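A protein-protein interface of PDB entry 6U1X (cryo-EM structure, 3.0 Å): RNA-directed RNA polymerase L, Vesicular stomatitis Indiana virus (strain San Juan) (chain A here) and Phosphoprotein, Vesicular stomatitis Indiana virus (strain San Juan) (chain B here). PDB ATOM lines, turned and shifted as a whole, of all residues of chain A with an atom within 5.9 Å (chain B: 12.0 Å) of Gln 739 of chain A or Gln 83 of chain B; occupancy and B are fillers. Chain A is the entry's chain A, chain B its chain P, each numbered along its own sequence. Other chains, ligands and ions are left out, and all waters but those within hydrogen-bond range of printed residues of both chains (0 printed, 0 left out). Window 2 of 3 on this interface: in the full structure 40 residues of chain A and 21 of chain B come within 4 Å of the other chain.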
ATOM      1  N   TYR A 722      -8.624  18.439 -12.376  1.00  0.00           N
ATOM      2  CA  TYR A 722      -8.138  17.736 -13.552  1.00  0.00           C
ATOM      3  C   TYR A 722      -7.934  18.732 -14.681  1.00  0.00           C
ATOM      4  O   TYR A 722      -8.567  19.788 -14.728  1.00  0.00           O
ATOM      5  CB  TYR A 722      -9.114  16.646 -14.013  1.00  0.00           C
ATOM      6  CG  TYR A 722      -9.350  15.554 -13.006  1.00  0.00           C
ATOM      7  CD1 TYR A 722      -8.567  14.414 -13.000  1.00  0.00           C
ATOM      8  CD2 TYR A 722     -10.360  15.660 -12.067  1.00  0.00           C
ATOM      9  CE1 TYR A 722      -8.778  13.413 -12.080  1.00  0.00           C
ATOM     10  CE2 TYR A 722     -10.580  14.663 -11.146  1.00  0.00           C
ATOM     11  CZ  TYR A 722      -9.786  13.542 -11.157  1.00  0.00           C
ATOM     12  OH  TYR A 722      -9.993  12.542 -10.242  1.00  0.00           O
ATOM     13  N   GLN A 734     -16.026  13.050 -24.017  1.00  0.00           N
ATOM     14  CA  GLN A 734     -16.957  12.396 -23.105  1.00  0.00           C
ATOM     15  C   GLN A 734     -16.289  11.228 -22.392  1.00  0.00           C
ATOM     16  O   GLN A 734     -16.538  10.996 -21.204  1.00  0.00           O
ATOM     17  CB  GLN A 734     -18.196  11.936 -23.868  1.00  0.00           C
ATOM     18  CG  GLN A 734     -19.477  12.010 -23.058  1.00  0.00           C
ATOM     19  CD  GLN A 734     -20.707  11.722 -23.892  1.00  0.00           C
ATOM     20  OE1 GLN A 734     -20.606  11.289 -25.039  1.00  0.00           O
ATOM     21  NE2 GLN A 734     -21.878  11.970 -23.320  1.00  0.00           N
ATOM     22  N   GLY A 735     -15.419  10.497 -23.091  1.00  0.00           N
ATOM     23  CA  GLY A 735     -14.678   9.432 -22.436  1.00  0.00           C
ATOM     24  C   GLY A 735     -13.738   9.958 -21.369  1.00  0.00           C
ATOM     25  O   GLY A 735     -13.604   9.369 -20.292  1.00  0.00           O
ATOM     26  N   ALA A 736     -13.072  11.076 -21.658  1.00  0.00           N
ATOM     27  CA  ALA A 736     -12.207  11.703 -20.668  1.00  0.00           C
ATOM     28  C   ALA A 736     -12.997  12.113 -19.437  1.00  0.00           C
ATOM     29  O   ALA A 736     -12.534  11.944 -18.304  1.00  0.00           O
ATOM     30  CB  ALA A 736     -11.512  12.914 -21.281  1.00  0.00           C
ATOM     31  N   LEU A 737     -14.197  12.652 -19.638  1.00  0.00           N
ATOM     32  CA  LEU A 737     -15.029  13.035 -18.501  1.00  0.00           C
ATOM     33  C   LEU A 737     -15.486  11.811 -17.714  1.00  0.00           C
ATOM     34  O   LEU A 737     -15.574  11.852 -16.476  1.00  0.00           O
ATOM     35  CB  LEU A 737     -16.224  13.846 -18.993  1.00  0.00           C
ATOM     36  CG  LEU A 737     -15.852  15.209 -19.582  1.00  0.00           C
ATOM     37  CD1 LEU A 737     -16.963  15.748 -20.442  1.00  0.00           C
ATOM     38  CD2 LEU A 737     -15.520  16.193 -18.481  1.00  0.00           C
ATOM     39  N   ASN A 738     -15.781  10.714 -18.414  1.00  0.00           N
ATOM     40  CA  ASN A 738     -16.101   9.466 -17.729  1.00  0.00           C
ATOM     41  C   ASN A 738     -14.945   9.029 -16.839  1.00  0.00           C
ATOM     42  O   ASN A 738     -15.150   8.636 -15.685  1.00  0.00           O
ATOM     43  CB  ASN A 738     -16.433   8.371 -18.744  1.00  0.00           C
ATOM     44  CG  ASN A 738     -17.613   8.723 -19.632  1.00  0.00           C
ATOM     45  OD1 ASN A 738     -17.547   8.579 -20.853  1.00  0.00           O
ATOM     46  ND2 ASN A 738     -18.702   9.179 -19.027  1.00  0.00           N
ATOM     47  N   GLN A 739     -13.719   9.101 -17.358  1.00  0.00           N
ATOM     48  CA  GLN A 739     -12.561   8.721 -16.554  1.00  0.00           C
ATOM     49  C   GLN A 739     -12.343   9.683 -15.392  1.00  0.00           C
ATOM     50  O   GLN A 739     -11.915   9.262 -14.309  1.00  0.00           O
ATOM     51  CB  GLN A 739     -11.315   8.654 -17.431  1.00  0.00           C
ATOM     52  CG  GLN A 739     -11.388   7.600 -18.522  1.00  0.00           C
ATOM     53  CD  GLN A 739     -11.516   6.195 -17.971  1.00  0.00           C
ATOM     54  OE1 GLN A 739     -10.891   5.850 -16.969  1.00  0.00           O
ATOM     55  NE2 GLN A 739     -12.339   5.381 -18.618  1.00  0.00           N
ATOM     56  N   MET A 740     -12.632  10.968 -15.596  1.00  0.00           N
ATOM     57  CA  MET A 740     -12.550  11.934 -14.505  1.00  0.00           C
ATOM     58  C   MET A 740     -13.472  11.538 -13.362  1.00  0.00           C
ATOM     59  O   MET A 740     -13.047  11.456 -12.201  1.00  0.00           O
ATOM     60  CB  MET A 740     -12.912  13.330 -15.012  1.00  0.00           C
ATOM     61  CG  MET A 740     -11.845  14.013 -15.831  1.00  0.00           C
ATOM     62  SD  MET A 740     -12.344  15.678 -16.304  1.00  0.00           S
ATOM     63  CE  MET A 740     -10.989  16.145 -17.372  1.00  0.00           C
ATOM     64  N   VAL A 741     -14.747  11.297 -13.670  1.00  0.00           N
ATOM     65  CA  VAL A 741     -15.691  10.952 -12.611  1.00  0.00           C
ATOM     66  C   VAL A 741     -15.343   9.598 -12.004  1.00  0.00           C
ATOM     67  O   VAL A 741     -15.576   9.368 -10.811  1.00  0.00           O
ATOM     68  CB  VAL A 741     -17.143  10.993 -13.129  1.00  0.00           C
ATOM     69  CG1 VAL A 741     -17.488  12.389 -13.601  1.00  0.00           C
ATOM     70  CG2 VAL A 741     -17.370  10.003 -14.249  1.00  0.00           C
ATOM     71  N   SER A 742     -14.768   8.690 -12.796  1.00  0.00           N
ATOM     72  CA  SER A 742     -14.331   7.408 -12.254  1.00  0.00           C
ATOM     73  C   SER A 742     -13.240   7.599 -11.208  1.00  0.00           C
ATOM     74  O   SER A 742     -13.309   7.034 -10.110  1.00  0.00           O
ATOM     75  CB  SER A 742     -13.840   6.506 -13.384  1.00  0.00           C
ATOM     76  OG  SER A 742     -14.881   6.231 -14.302  1.00  0.00           O
ATOM     77  N   ASN A 743     -12.218   8.391 -11.532  1.00  0.00           N
ATOM     78  CA  ASN A 743     -11.150   8.646 -10.571  1.00  0.00           C
ATOM     79  C   ASN A 743     -11.685   9.364  -9.336  1.00  0.00           C
ATOM     80  O   ASN A 743     -11.248   9.098  -8.205  1.00  0.00           O
ATOM     81  CB  ASN A 743     -10.045   9.463 -11.235  1.00  0.00           C
ATOM     82  CG  ASN A 743      -8.803   9.575 -10.379  1.00  0.00           C
ATOM     83  OD1 ASN A 743      -8.753  10.365  -9.438  1.00  0.00           O
ATOM     84  ND2 ASN A 743      -7.786   8.791 -10.709  1.00  0.00           N
ATOM     85  N   ASN A 744     -12.643  10.273  -9.534  1.00  0.00           N
ATOM     86  CA  ASN A 744     -13.231  10.986  -8.406  1.00  0.00           C
ATOM     87  C   ASN A 744     -13.945  10.024  -7.465  1.00  0.00           C
ATOM     88  O   ASN A 744     -13.740  10.063  -6.244  1.00  0.00           O
ATOM     89  CB  ASN A 744     -14.189  12.062  -8.916  1.00  0.00           C
ATOM     90  CG  ASN A 744     -14.566  13.061  -7.845  1.00  0.00           C
ATOM     91  OD1 ASN A 744     -13.794  13.963  -7.525  1.00  0.00           O
ATOM     92  ND2 ASN A 744     -15.762  12.915  -7.293  1.00  0.00           N
ATOM     93  N   ILE A2094      -4.514   8.439 -27.327  1.00  0.00           N
ATOM     94  CA  ILE A2094      -5.727   8.813 -26.612  1.00  0.00           C
ATOM     95  C   ILE A2094      -5.528  10.201 -26.028  1.00  0.00           C
ATOM     96  O   ILE A2094      -4.401  10.666 -25.844  1.00  0.00           O
ATOM     97  CB  ILE A2094      -6.077   7.804 -25.497  1.00  0.00           C
ATOM     98  CG1 ILE A2094      -4.834   7.481 -24.671  1.00  0.00           C
ATOM     99  CG2 ILE A2094      -6.666   6.541 -26.094  1.00  0.00           C
ATOM    100  CD1 ILE A2094      -5.147   6.899 -23.329  1.00  0.00           C
ATOM    101  N   LEU A2095      -6.639  10.866 -25.729  1.00  0.00           N
ATOM    102  CA  LEU A2095      -6.568  12.180 -25.110  1.00  0.00           C
ATOM    103  C   LEU A2095      -5.954  12.063 -23.724  1.00  0.00           C
ATOM    104  O   LEU A2095      -6.363  11.223 -22.918  1.00  0.00           O
ATOM    105  CB  LEU A2095      -7.959  12.800 -25.029  1.00  0.00           C
ATOM    106  CG  LEU A2095      -8.035  14.226 -24.487  1.00  0.00           C
ATOM    107  CD1 LEU A2095      -7.283  15.180 -25.388  1.00  0.00           C
ATOM    108  CD2 LEU A2095      -9.477  14.646 -24.352  1.00  0.00           C
ATOM    109  N   MET A2096      -4.971  12.912 -23.448  1.00  0.00           N
ATOM    110  CA  MET A2096      -4.227  12.822 -22.205  1.00  0.00           C
ATOM    111  C   MET A2096      -4.970  13.527 -21.078  1.00  0.00           C
ATOM    112  O   MET A2096      -5.691  14.505 -21.290  1.00  0.00           O
ATOM    113  CB  MET A2096      -2.836  13.430 -22.372  1.00  0.00           C
ATOM    114  CG  MET A2096      -1.943  13.340 -21.138  1.00  0.00           C
ATOM    115  SD  MET A2096      -1.816  11.691 -20.412  1.00  0.00           S
ATOM    116  CE  MET A2096      -1.408  10.706 -21.851  1.00  0.00           C
ATOM    117  N   LEU A2097      -4.782  13.010 -19.866  1.00  0.00           N
ATOM    118  CA  LEU A2097      -5.408  13.551 -18.673  1.00  0.00           C
ATOM    119  C   LEU A2097      -4.387  13.591 -17.550  1.00  0.00           C
ATOM    120  O   LEU A2097      -3.344  12.936 -17.606  1.00  0.00           O
ATOM    121  CB  LEU A2097      -6.618  12.717 -18.255  1.00  0.00           C
ATOM    122  CG  LEU A2097      -7.855  12.917 -19.120  1.00  0.00           C
ATOM    123  CD1 LEU A2097      -8.569  11.603 -19.346  1.00  0.00           C
ATOM    124  CD2 LEU A2097      -8.768  13.923 -18.453  1.00  0.00           C
ATOM    125  N   GLU B  82      -4.282   3.152 -15.653  1.00  0.00           N
ATOM    126  CA  GLU B  82      -5.519   3.910 -15.807  1.00  0.00           C
ATOM    127  C   GLU B  82      -5.397   4.902 -16.958  1.00  0.00           C
ATOM    128  O   GLU B  82      -4.376   4.947 -17.645  1.00  0.00           O
ATOM    129  CB  GLU B  82      -5.865   4.646 -14.509  1.00  0.00           C
ATOM    130  CG  GLU B  82      -6.010   3.743 -13.293  1.00  0.00           C
ATOM    131  CD  GLU B  82      -7.187   2.793 -13.401  1.00  0.00           C
ATOM    132  OE1 GLU B  82      -8.019   2.973 -14.315  1.00  0.00           O
ATOM    133  OE2 GLU B  82      -7.282   1.865 -12.571  1.00  0.00           O
ATOM    134  N   GLN B  83      -6.448   5.694 -17.162  1.00  0.00           N
ATOM    135  CA  GLN B  83      -6.470   6.688 -18.226  1.00  0.00           C
ATOM    136  C   GLN B  83      -5.953   8.044 -17.771  1.00  0.00           C
ATOM    137  O   GLN B  83      -5.380   8.782 -18.581  1.00  0.00           O
ATOM    138  CB  GLN B  83      -7.891   6.843 -18.771  1.00  0.00           C
ATOM    139  CG  GLN B  83      -8.452   5.586 -19.423  1.00  0.00           C
ATOM    140  CD  GLN B  83      -7.758   5.240 -20.719  1.00  0.00           C
ATOM    141  OE1 GLN B  83      -6.917   5.992 -21.204  1.00  0.00           O
ATOM    142  NE2 GLN B  83      -8.110   4.096 -21.291  1.00  0.00           N
ATOM    143  N   VAL B  84      -6.142   8.387 -16.500  1.00  0.00           N
ATOM    144  CA  VAL B  84      -5.667   9.652 -15.952  1.00  0.00           C
ATOM    145  C   VAL B  84      -4.308   9.432 -15.306  1.00  0.00           C
ATOM    146  O   VAL B  84      -4.131   8.513 -14.498  1.00  0.00           O
ATOM    147  CB  VAL B  84      -6.673  10.236 -14.942  1.00  0.00           C
ATOM    148  CG1 VAL B  84      -8.015  10.446 -15.593  1.00  0.00           C
ATOM    149  CG2 VAL B  84      -6.815   9.355 -13.711  1.00  0.00           C
ATOM    150  N   GLU B  85      -3.343  10.268 -15.674  1.00  0.00           N
ATOM    151  CA  GLU B  85      -2.021  10.202 -15.076  1.00  0.00           C
ATOM    152  C   GLU B  85      -2.044  10.831 -13.689  1.00  0.00           C
ATOM    153  O   GLU B  85      -2.812  11.755 -13.413  1.00  0.00           O
ATOM    154  CB  GLU B  85      -0.994  10.916 -15.954  1.00  0.00           C
ATOM    155  CG  GLU B  85      -0.873  10.356 -17.364  1.00  0.00           C
ATOM    156  CD  GLU B  85      -0.354   8.929 -17.393  1.00  0.00           C
ATOM    157  OE1 GLU B  85       0.158   8.456 -16.357  1.00  0.00           O
ATOM    158  OE2 GLU B  85      -0.459   8.280 -18.455  1.00  0.00           O
ATOM    159  N   GLY B  86      -1.190  10.315 -12.815  1.00  0.00           N
ATOM    160  CA  GLY B  86      -1.135  10.785 -11.452  1.00  0.00           C
ATOM    161  C   GLY B  86      -0.680  12.226 -11.353  1.00  0.00           C
ATOM    162  O   GLY B  86      -0.375  12.900 -12.336  1.00  0.00           O
ATOM    163  N   PHE B  87      -0.636  12.702 -10.112  1.00  0.00           N
ATOM    164  CA  PHE B  87      -0.250  14.076  -9.821  1.00  0.00           C
ATOM    165  C   PHE B  87       1.256  14.240  -9.673  1.00  0.00           C
ATOM    166  O   PHE B  87       1.789  15.305 -10.006  1.00  0.00           O
ATOM    167  CB  PHE B  87      -0.956  14.547  -8.548  1.00  0.00           C
ATOM    168  CG  PHE B  87      -0.498  15.884  -8.051  1.00  0.00           C
ATOM    169  CD1 PHE B  87      -0.455  16.978  -8.896  1.00  0.00           C
ATOM    170  CD2 PHE B  87      -0.132  16.051  -6.730  1.00  0.00           C
ATOM    171  CE1 PHE B  87      -0.038  18.206  -8.434  1.00  0.00           C
ATOM    172  CE2 PHE B  87       0.282  17.276  -6.264  1.00  0.00           C
ATOM    173  CZ  PHE B  87       0.331  18.354  -7.115  1.00  0.00           C
ATOM    174  N   GLN B  89       5.070  12.625 -10.610  1.00  0.00           N
ATOM    175  CA  GLN B  89       5.763  11.759 -11.555  1.00  0.00           C
ATOM    176  C   GLN B  89       7.266  12.014 -11.511  1.00  0.00           C
ATOM    177  O   GLN B  89       8.049  11.116 -11.199  1.00  0.00           O
ATOM    178  CB  GLN B  89       5.234  11.982 -12.973  1.00  0.00           C
ATOM    179  CG  GLN B  89       3.857  11.396 -13.229  1.00  0.00           C
ATOM    180  CD  GLN B  89       3.879   9.887 -13.365  1.00  0.00           C
ATOM    181  OE1 GLN B  89       4.921   9.252 -13.205  1.00  0.00           O
ATOM    182  NE2 GLN B  89       2.725   9.306 -13.666  1.00  0.00           N
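O of Leu 2097 of chain A is in hydrogen-bond range of N of Glu 85 of chain B, 3.3 Å away.
OH of Tyr 722 of chain A is in hydrogen-bond range of OD1 of Asn 743 of chain A, at 2.6 Å.
Among the printed residues, pairs that only touch across the chains: Gln 739 of chain A with Gln 83 of chain B (3.4 Å), Asn 743 of chain A with Val 84 of chain B (3.2 Å), Ile 2094 of chain A with Gln 83 of chain B (2.9 Å), Met 2096 of chain A with Glu 85 of chain B (3.5 Å) and Leu 2097 of chain A with Val 84 of chain B (3.8 Å).
No residue of chain B comes within 4 Å of Ala 736 of chain A. No residue of chain B comes within 4 Å of Asn 738 of chain A. Of chain B, only Gln 83 comes within 4 Å of Gln 739 of chain A. No residue of chain B comes within 4 Å of Met 740 of chain A. No residue of chain B comes within 4 Å of Val 741 of chain A. Ser 742 of chain A touches none of the printed residues of chain B. Asn 743 of chain A touches just one residue of chain B: Val 84. Of the printed residues of chain A, Val 84 of chain B touches Asn 743 (3.2 Å) and Leu 2097 (3.8 Å). Printed residues of chain A within 4 Å of Glu 85 of chain B: Met 2096 (3.5 Å) and Leu 2097 (3.3 Å). The nearest printed residue of chain A that does not touch Glu 85 of chain B is Tyr 722 of chain A (6.3 Å).
Printed residues of chain A that touch a printed residue of chain B: Gln 739, Asn 743, Ile 2094, Met 2096 and Leu 2097. Printed residues of chain B that touch a printed residue of chain A: Gln 83, Val 84 and Glu 85. Among the printed residues, no Asp or Glu carboxylate lies within 4 Å of a Lys or Arg side-chain nitrogen of the other chain.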
